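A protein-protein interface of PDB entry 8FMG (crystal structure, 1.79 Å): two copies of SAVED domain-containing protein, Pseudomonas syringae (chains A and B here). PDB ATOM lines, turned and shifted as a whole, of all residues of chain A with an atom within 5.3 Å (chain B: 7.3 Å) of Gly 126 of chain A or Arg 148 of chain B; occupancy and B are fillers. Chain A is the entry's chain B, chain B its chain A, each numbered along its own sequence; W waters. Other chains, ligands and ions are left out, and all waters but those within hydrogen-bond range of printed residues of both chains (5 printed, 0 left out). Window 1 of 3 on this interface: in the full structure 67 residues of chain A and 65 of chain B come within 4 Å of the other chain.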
ATOM      1  N   LEU A 119     -28.737   5.465  22.942  1.00  0.00           N
ATOM      2  CA  LEU A 119     -29.082   6.780  23.465  1.00  0.00           C
ATOM      3  C   LEU A 119     -29.911   6.652  24.738  1.00  0.00           C
ATOM      4  O   LEU A 119     -29.632   7.321  25.740  1.00  0.00           O
ATOM      5  CB  LEU A 119     -29.824   7.577  22.397  1.00  0.00           C
ATOM      6  CG  LEU A 119     -30.105   9.049  22.690  1.00  0.00           C
ATOM      7  CD1 LEU A 119     -28.824   9.811  22.915  1.00  0.00           C
ATOM      8  CD2 LEU A 119     -30.867   9.662  21.536  1.00  0.00           C
ATOM      9  N   THR A 122     -28.010   4.912  27.891  1.00  0.00           N
ATOM     10  CA  THR A 122     -26.992   5.767  28.484  1.00  0.00           C
ATOM     11  C   THR A 122     -27.573   7.034  29.093  1.00  0.00           C
ATOM     12  O   THR A 122     -26.814   7.858  29.613  1.00  0.00           O
ATOM     13  CB  THR A 122     -25.943   6.153  27.438  1.00  0.00           C
ATOM     14  OG1 THR A 122     -26.580   6.841  26.356  1.00  0.00           O
ATOM     15  CG2 THR A 122     -25.235   4.923  26.903  1.00  0.00           C
ATOM     16  N   THR A 123     -28.894   7.205  29.039  1.00  0.00           N
ATOM     17  CA  THR A 123     -29.499   8.443  29.514  1.00  0.00           C
ATOM     18  C   THR A 123     -29.160   8.761  30.967  1.00  0.00           C
ATOM     19  O   THR A 123     -29.118   9.957  31.303  1.00  0.00           O
ATOM     20  CB  THR A 123     -31.022   8.373  29.318  1.00  0.00           C
ATOM     21  OG1 THR A 123     -31.328   8.516  27.921  1.00  0.00           O
ATOM     22  CG2 THR A 123     -31.743   9.467  30.086  1.00  0.00           C
ATOM     23  N   PRO A 124     -28.926   7.794  31.853  1.00  0.00           N
ATOM     24  CA  PRO A 124     -28.538   8.162  33.223  1.00  0.00           C
ATOM     25  C   PRO A 124     -27.292   9.029  33.296  1.00  0.00           C
ATOM     26  O   PRO A 124     -27.180   9.838  34.226  1.00  0.00           O
ATOM     27  CB  PRO A 124     -28.343   6.800  33.903  1.00  0.00           C
ATOM     28  CG  PRO A 124     -29.298   5.901  33.174  1.00  0.00           C
ATOM     29  CD  PRO A 124     -29.236   6.354  31.735  1.00  0.00           C
ATOM     30  N   ASP A 125     -26.354   8.913  32.353  1.00  0.00           N
ATOM     31  CA  ASP A 125     -25.160   9.757  32.419  1.00  0.00           C
ATOM     32  C   ASP A 125     -25.451  11.197  32.012  1.00  0.00           C
ATOM     33  O   ASP A 125     -24.586  12.059  32.186  1.00  0.00           O
ATOM     34  CB  ASP A 125     -24.016   9.155  31.582  1.00  0.00           C
ATOM     35  CG  ASP A 125     -24.039   9.560  30.105  1.00  0.00           C
ATOM     36  OD1 ASP A 125     -24.758  10.497  29.714  1.00  0.00           O
ATOM     37  OD2 ASP A 125     -23.309   8.927  29.309  1.00  0.00           O
ATOM     38  N   GLY A 126     -26.635  11.470  31.458  1.00  0.00           N
ATOM     39  CA  GLY A 126     -27.062  12.835  31.234  1.00  0.00           C
ATOM     40  C   GLY A 126     -27.357  13.604  32.502  1.00  0.00           C
ATOM     41  O   GLY A 126     -27.594  14.816  32.436  1.00  0.00           O
ATOM     42  N   GLY A 127     -27.340  12.929  33.644  1.00  0.00           N
ATOM     43  CA  GLY A 127     -27.585  13.546  34.924  1.00  0.00           C
ATOM     44  C   GLY A 127     -26.364  14.004  35.676  1.00  0.00           C
ATOM     45  O   GLY A 127     -26.494  14.447  36.818  1.00  0.00           O
ATOM     46  N   ARG A 128     -25.167  13.902  35.088  1.00  0.00           N
ATOM     47  CA  ARG A 128     -23.978  14.450  35.726  1.00  0.00           C
ATOM     48  C   ARG A 128     -24.230  15.912  36.080  1.00  0.00           C
ATOM     49  O   ARG A 128     -24.778  16.674  35.283  1.00  0.00           O
ATOM     50  CB  ARG A 128     -22.759  14.314  34.812  1.00  0.00           C
ATOM     51  CG  ARG A 128     -22.297  12.865  34.600  1.00  0.00           C
ATOM     52  CD  ARG A 128     -21.012  12.758  33.760  1.00  0.00           C
ATOM     53  NE  ARG A 128     -19.804  13.115  34.497  1.00  0.00           N
ATOM     54  CZ  ARG A 128     -19.194  14.293  34.431  1.00  0.00           C
ATOM     55  NH1 ARG A 128     -19.641  15.262  33.647  1.00  0.00           N
ATOM     56  NH2 ARG A 128     -18.108  14.505  35.173  1.00  0.00           N
ATOM     57  N   THR A 204     -21.335  10.463  27.728  1.00  0.00           N
ATOM     58  CA  THR A 204     -21.286   9.855  26.405  1.00  0.00           C
ATOM     59  C   THR A 204     -20.855  10.837  25.322  1.00  0.00           C
ATOM     60  O   THR A 204     -20.231  10.424  24.336  1.00  0.00           O
ATOM     61  CB  THR A 204     -22.658   9.272  26.056  1.00  0.00           C
ATOM     62  OG1 THR A 204     -23.013   8.265  27.009  1.00  0.00           O
ATOM     63  CG2 THR A 204     -22.656   8.674  24.660  1.00  0.00           C
ATOM     64  N   TYR A 205     -21.186  12.120  25.462  1.00  0.00           N
ATOM     65  CA  TYR A 205     -20.970  13.076  24.387  1.00  0.00           C
ATOM     66  C   TYR A 205     -20.073  14.244  24.765  1.00  0.00           C
ATOM     67  O   TYR A 205     -19.854  15.131  23.931  1.00  0.00           O
ATOM     68  CB  TYR A 205     -22.321  13.610  23.881  1.00  0.00           C
ATOM     69  CG  TYR A 205     -23.235  12.508  23.401  1.00  0.00           C
ATOM     70  CD1 TYR A 205     -22.974  11.840  22.216  1.00  0.00           C
ATOM     71  CD2 TYR A 205     -24.352  12.119  24.138  1.00  0.00           C
ATOM     72  CE1 TYR A 205     -23.791  10.825  21.769  1.00  0.00           C
ATOM     73  CE2 TYR A 205     -25.181  11.098  23.695  1.00  0.00           C
ATOM     74  CZ  TYR A 205     -24.892  10.453  22.504  1.00  0.00           C
ATOM     75  OH  TYR A 205     -25.689   9.437  22.032  1.00  0.00           O
ATOM     76  N   ASP A 207     -20.683  16.459  27.248  1.00  0.00           N
ATOM     77  CA  ASP A 207     -21.464  17.614  27.660  1.00  0.00           C
ATOM     78  C   ASP A 207     -20.971  18.149  29.004  1.00  0.00           C
ATOM     79  O   ASP A 207     -20.517  17.401  29.874  1.00  0.00           O
ATOM     80  CB  ASP A 207     -22.950  17.260  27.774  1.00  0.00           C
ATOM     81  CG  ASP A 207     -23.674  17.240  26.424  1.00  0.00           C
ATOM     82  OD1 ASP A 207     -23.251  17.944  25.484  1.00  0.00           O
ATOM     83  OD2 ASP A 207     -24.692  16.524  26.317  1.00  0.00           O
ATOM     84  N   LYS A 234     -28.221  23.641  31.095  1.00  0.00           N
ATOM     85  CA  LYS A 234     -28.918  22.632  31.888  1.00  0.00           C
ATOM     86  C   LYS A 234     -28.720  22.976  33.362  1.00  0.00           C
ATOM     87  O   LYS A 234     -27.628  22.786  33.908  1.00  0.00           O
ATOM     88  CB  LYS A 234     -28.426  21.225  31.579  1.00  0.00           C
ATOM     89  CG  LYS A 234     -29.385  20.172  32.116  1.00  0.00           C
ATOM     90  CD  LYS A 234     -28.970  18.763  31.757  1.00  0.00           C
ATOM     91  CE  LYS A 234     -29.977  17.762  32.312  1.00  0.00           C
ATOM     92  NZ  LYS A 234     -29.759  16.382  31.803  1.00  0.00           N
ATOM     93  N   CYS B  35     -26.388   4.747  36.353  1.00  0.00           N
ATOM     94  CA  CYS B  35     -25.302   5.532  35.778  1.00  0.00           C
ATOM     95  C   CYS B  35     -25.148   5.349  34.278  1.00  0.00           C
ATOM     96  O   CYS B  35     -24.348   6.066  33.668  1.00  0.00           O
ATOM     97  CB  CYS B  35     -23.967   5.197  36.459  1.00  0.00           C
ATOM     98  SG  CYS B  35     -23.193   3.624  35.991  1.00  0.00           S
ATOM     99  N   GLY B  36     -25.872   4.420  33.666  1.00  0.00           N
ATOM    100  CA  GLY B  36     -25.863   4.318  32.225  1.00  0.00           C
ATOM    101  C   GLY B  36     -24.638   3.681  31.611  1.00  0.00           C
ATOM    102  O   GLY B  36     -24.506   3.710  30.384  1.00  0.00           O
ATOM    103  N   ILE B 133     -25.536  22.522  16.472  1.00  0.00           N
ATOM    104  CA  ILE B 133     -25.742  23.425  17.598  1.00  0.00           C
ATOM    105  C   ILE B 133     -24.912  24.675  17.345  1.00  0.00           C
ATOM    106  O   ILE B 133     -23.714  24.580  17.044  1.00  0.00           O
ATOM    107  CB  ILE B 133     -25.328  22.767  18.922  1.00  0.00           C
ATOM    108  CG1 ILE B 133     -26.271  21.624  19.292  1.00  0.00           C
ATOM    109  CG2 ILE B 133     -25.304  23.792  20.045  1.00  0.00           C
ATOM    110  CD1 ILE B 133     -25.699  20.701  20.352  1.00  0.00           C
ATOM    111  N   ILE B 145     -25.779  24.544  25.131  1.00  0.00           N
ATOM    112  CA  ILE B 145     -26.846  23.639  24.717  1.00  0.00           C
ATOM    113  C   ILE B 145     -26.297  22.216  24.746  1.00  0.00           C
ATOM    114  O   ILE B 145     -25.390  21.904  23.960  1.00  0.00           O
ATOM    115  CB  ILE B 145     -27.370  23.995  23.316  1.00  0.00           C
ATOM    116  CG1 ILE B 145     -27.859  25.440  23.318  1.00  0.00           C
ATOM    117  CG2 ILE B 145     -28.438  23.004  22.911  1.00  0.00           C
ATOM    118  CD1 ILE B 145     -28.366  25.907  21.989  1.00  0.00           C
ATOM    119  N   PRO B 146     -26.823  21.332  25.592  1.00  0.00           N
ATOM    120  CA  PRO B 146     -26.243  19.989  25.683  1.00  0.00           C
ATOM    121  C   PRO B 146     -26.479  19.189  24.412  1.00  0.00           C
ATOM    122  O   PRO B 146     -27.579  19.183  23.854  1.00  0.00           O
ATOM    123  CB  PRO B 146     -26.964  19.361  26.886  1.00  0.00           C
ATOM    124  CG  PRO B 146     -27.664  20.505  27.584  1.00  0.00           C
ATOM    125  CD  PRO B 146     -27.959  21.510  26.516  1.00  0.00           C
ATOM    126  N   VAL B 147     -25.425  18.504  23.959  1.00  0.00           N
ATOM    127  CA  VAL B 147     -25.542  17.651  22.778  1.00  0.00           C
ATOM    128  C   VAL B 147     -26.569  16.551  23.013  1.00  0.00           C
ATOM    129  O   VAL B 147     -27.368  16.230  22.124  1.00  0.00           O
ATOM    130  CB  VAL B 147     -24.165  17.067  22.408  1.00  0.00           C
ATOM    131  CG1 VAL B 147     -24.306  15.926  21.405  1.00  0.00           C
ATOM    132  CG2 VAL B 147     -23.251  18.152  21.850  1.00  0.00           C
ATOM    133  N   ARG B 148     -26.559  15.944  24.203  1.00  0.00           N
ATOM    134  CA  ARG B 148     -27.481  14.842  24.455  1.00  0.00           C
ATOM    135  C   ARG B 148     -28.929  15.277  24.244  1.00  0.00           C
ATOM    136  O   ARG B 148     -29.737  14.517  23.704  1.00  0.00           O
ATOM    137  CB  ARG B 148     -27.297  14.292  25.872  1.00  0.00           C
ATOM    138  CG  ARG B 148     -28.389  13.298  26.273  1.00  0.00           C
ATOM    139  CD  ARG B 148     -28.138  12.629  27.623  1.00  0.00           C
ATOM    140  NE  ARG B 148     -27.032  11.682  27.565  1.00  0.00           N
ATOM    141  CZ  ARG B 148     -27.106  10.477  27.014  1.00  0.00           C
ATOM    142  NH1 ARG B 148     -28.229  10.033  26.466  1.00  0.00           N
ATOM    143  NH2 ARG B 148     -26.027   9.702  27.002  1.00  0.00           N
ATOM    144  N   ASP B 149     -29.273  16.497  24.655  1.00  0.00           N
ATOM    145  CA  ASP B 149     -30.669  16.927  24.584  1.00  0.00           C
ATOM    146  C   ASP B 149     -31.119  17.100  23.136  1.00  0.00           C
ATOM    147  O   ASP B 149     -32.241  16.719  22.785  1.00  0.00           O
ATOM    148  CB  ASP B 149     -30.862  18.211  25.401  1.00  0.00           C
ATOM    149  CG  ASP B 149     -30.750  17.968  26.914  1.00  0.00           C
ATOM    150  OD1 ASP B 149     -29.626  17.740  27.407  1.00  0.00           O
ATOM    151  OD2 ASP B 149     -31.786  18.001  27.614  1.00  0.00           O
ATOM    152  N   LEU B 150     -30.256  17.634  22.269  1.00  0.00           N
ATOM    153  CA  LEU B 150     -30.599  17.683  20.851  1.00  0.00           C
ATOM    154  C   LEU B 150     -30.742  16.276  20.278  1.00  0.00           C
ATOM    155  O   LEU B 150     -31.703  15.979  19.556  1.00  0.00           O
ATOM    156  CB  LEU B 150     -29.545  18.474  20.074  1.00  0.00           C
ATOM    157  CG  LEU B 150     -29.764  18.461  18.558  1.00  0.00           C
ATOM    158  CD1 LEU B 150     -31.107  19.082  18.217  1.00  0.00           C
ATOM    159  CD2 LEU B 150     -28.659  19.189  17.825  1.00  0.00           C
ATOM    160  N   LEU B 151     -29.786  15.390  20.589  1.00  0.00           N
ATOM    161  CA  LEU B 151     -29.837  14.035  20.049  1.00  0.00           C
ATOM    162  C   LEU B 151     -31.085  13.300  20.518  1.00  0.00           C
ATOM    163  O   LEU B 151     -31.646  12.485  19.772  1.00  0.00           O
ATOM    164  CB  LEU B 151     -28.590  13.255  20.462  1.00  0.00           C
ATOM    165  CG  LEU B 151     -27.262  13.642  19.805  1.00  0.00           C
ATOM    166  CD1 LEU B 151     -26.111  12.836  20.401  1.00  0.00           C
ATOM    167  CD2 LEU B 151     -27.326  13.447  18.298  1.00  0.00           C
ATOM    168  N   THR B 152     -31.526  13.580  21.747  1.00  0.00           N
ATOM    169  CA  THR B 152     -32.725  12.952  22.281  1.00  0.00           C
ATOM    170  C   THR B 152     -33.978  13.526  21.638  1.00  0.00           C
ATOM    171  O   THR B 152     -34.963  12.809  21.425  1.00  0.00           O
ATOM    172  CB  THR B 152     -32.775  13.145  23.793  1.00  0.00           C
ATOM    173  OG1 THR B 152     -31.660  12.475  24.397  1.00  0.00           O
ATOM    174  CG2 THR B 152     -34.078  12.607  24.360  1.00  0.00           C
ATOM    175  N   ALA B 153     -33.972  14.830  21.360  1.00  0.00           N
ATOM    176  CA  ALA B 153     -35.073  15.409  20.604  1.00  0.00           C
ATOM    177  C   ALA B 153     -35.152  14.788  19.217  1.00  0.00           C
ATOM    178  O   ALA B 153     -36.243  14.462  18.735  1.00  0.00           O
ATOM    179  CB  ALA B 153     -34.909  16.925  20.517  1.00  0.00           C
ATOM    180  N   MET B 154     -34.001  14.593  18.564  1.00  0.00           N
ATOM    181  CA  MET B 154     -34.001  13.968  17.246  1.00  0.00           C
ATOM    182  C   MET B 154     -34.556  12.553  17.313  1.00  0.00           C
ATOM    183  O   MET B 154     -35.415  12.167  16.513  1.00  0.00           O
ATOM    184  CB  MET B 154     -32.583  13.942  16.676  1.00  0.00           C
ATOM    185  CG  MET B 154     -31.999  15.299  16.368  1.00  0.00           C
ATOM    186  SD  MET B 154     -30.269  15.203  15.858  1.00  0.00           S
ATOM    187  CE  MET B 154     -30.316  13.885  14.640  1.00  0.00           C
ATOM    188  N   GLN B 164     -22.170  12.669  16.792  1.00  0.00           N
ATOM    189  CA  GLN B 164     -22.849  13.674  17.600  1.00  0.00           C
ATOM    190  C   GLN B 164     -22.970  15.027  16.906  1.00  0.00           C
ATOM    191  O   GLN B 164     -23.642  15.919  17.436  1.00  0.00           O
ATOM    192  CB  GLN B 164     -22.151  13.838  18.955  1.00  0.00           C
ATOM    193  CG  GLN B 164     -20.834  14.581  18.967  1.00  0.00           C
ATOM    194  CD  GLN B 164     -20.313  14.761  20.386  1.00  0.00           C
ATOM    195  OE1 GLN B 164     -20.323  15.860  20.934  1.00  0.00           O
ATOM    196  NE2 GLN B 164     -19.875  13.661  20.994  1.00  0.00           N
ATOM    197  N   LEU B 246     -34.724  21.145  25.271  1.00  0.00           N
ATOM    198  CA  LEU B 246     -34.991  20.798  23.878  1.00  0.00           C
ATOM    199  C   LEU B 246     -36.310  20.059  23.680  1.00  0.00           C
ATOM    200  O   LEU B 246     -36.708  19.826  22.532  1.00  0.00           O
ATOM    201  CB  LEU B 246     -33.845  19.952  23.306  1.00  0.00           C
ATOM    202  CG  LEU B 246     -32.741  20.724  22.586  1.00  0.00           C
ATOM    203  CD1 LEU B 246     -33.210  21.262  21.244  1.00  0.00           C
ATOM    204  CD2 LEU B 246     -32.247  21.874  23.445  1.00  0.00           C
HETATM  205  O   HOH W   1     -19.334  17.950  23.342  1.00  0.00           O
HETATM  206  O   HOH W   2     -30.865  11.007  26.641  1.00  0.00           O
HETATM  207  O   HOH W   3     -28.687  15.999  29.261  1.00  0.00           O
HETATM  208  O   HOH W   4     -31.945  16.948  29.865  1.00  0.00           O
HETATM  209  O   HOH W   5     -24.695  13.078  28.668  1.00  0.00           O
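The backbone NH (N) of Val 147 of chain B lies within hydrogen-bond range of the side-chain carboxylate (OD1) of Asp 207 of chain A (2.7 Å). The guanidinium group of Arg 148 of chain B sits at hydrogen-bond distance from the backbone carbonyl oxygen of Leu 119 of chain A. NH2 of Arg 148 of chain B lies within hydrogen-bond range of OG1 of Thr 122 of chain A, at 3.0 Å. OD1 of Asp 125 of chain A is in salt-bridge range of NH2 of Arg 148 of chain B. The guanidinium group of Arg 148 of chain B lies within hydrogen-bond range of the side-chain hydroxyl of Thr 204 of chain A (3.3 Å). The backbone NH (N) of Arg 148 of chain B lies within hydrogen-bond range of the side-chain carboxylate (OD2) of Asp 207 of chain A (2.9 Å). The side-chain amide oxygen of Gln 164 of chain B sits close to the backbone carbonyl oxygen of Tyr 205 of chain A (3.1 Å).
The backbone carbonyl oxygen (O) of Arg 148 of chain B lies within hydrogen-bond range of the side-chain hydroxyl (OG1) of Thr 152 of chain B. O of Leu 119 of chain A lies within hydrogen-bond range of OG1 of Thr 122 of chain A, 3.2 Å away. The backbone carbonyl oxygen (O) of Leu 119 of chain A lies within hydrogen-bond range of the side-chain hydroxyl (OG1) of Thr 123 of chain A (3.0 Å). The side-chain carboxylate (OD2) of Asp 125 of chain A lies within hydrogen-bond range of the side-chain hydroxyl (OG1) of Thr 204 of chain A, 2.4 Å away. O of Gly 126 of chain A sits at hydrogen-bond distance from NZ of Lys 234 of chain A (2.7 Å).
Among the printed residues, merely in contact across the chains: Tyr 205 of chain A with Leu 151 of chain B (3.4 Å), Leu 119 of chain A with Leu 151 of chain B (3.4 Å), Pro 124 of chain A with Gly 36 of chain B (3.4 Å), Pro 124 of chain A with Cys 35 of chain B (3.5 Å), Asp 207 of chain A with Pro 146 of chain B (3.6 Å), Thr 123 of chain A with Arg 148 of chain B (3.7 Å), Tyr 205 of chain A with Arg 148 of chain B (3.7 Å), Asp 125 of chain A with Cys 35 of chain B (3.7 Å), Thr 122 of chain A with Gly 36 of chain B (3.7 Å), Gly 126 of chain A with Arg 148 of chain B (3.8 Å), Leu 119 of chain A with Thr 152 of chain B (3.9 Å) and Tyr 205 of chain A with Val 147 of chain B (3.9 Å).
Of the printed residues of chain B, Asp 207 of chain A touches Pro 146 (3.6 Å), Val 147 (2.7 Å) and Arg 148 (2.9 Å). Of the printed residues of chain A, Gly 36 of chain B touches Thr 122 (3.7 Å) and Pro 124 (3.4 Å). Of the printed residues of chain A, Pro 146 of chain B touches Asp 207 (3.6 Å). Printed residues of chain A within 4 Å of Val 147 of chain B: Tyr 205 (3.9 Å) and Asp 207 (2.7 Å). Of the printed residues of chain A, Leu 151 of chain B touches Leu 119 and Tyr 205. The nearest printed residue of chain A that does not touch Cys 35 of chain B is Thr 122 of chain A (5.1 Å).
Hydrophobic or aromatic side chains of chain A that line the printed part of chain B: Leu 119, Pro 124 and Tyr 205. Among the printed residues, 19 pairs touch across the chains.
No position is printed for both chains. Of the 19 pairs that touch across the chains among the printed residues, none has its exchanged pair printed and touching as well.
Water W4 bridges the side-chain carboxylate (OD2) of Asp 149 of chain B (2.5 Å) and the side-chain amino group (NZ) of Lys 234 of chain A (3.0 Å). Water W3 lies within hydrogen-bond range of the side-chain carboxylate (OD1) of Asp 149 of chain B (2.7 Å) and the side-chain amino group (NZ) of Lys 234 of chain A (2.8 Å). Water W5 bridges OD1 of Asp 125 of chain A (2.8 Å) and NE of Arg 148 of chain B (2.9 Å). Water W2 lies within hydrogen-bond range of OG1 of Thr 152 of chain B, NH1 of Arg 148 of chain B and OG1 of Thr 123 of chain A. Water W1 lies within hydrogen-bond range of O of Tyr 205 of chain A (2.9 Å) and OE1 of Gln 164 of chain B (3.3 Å).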
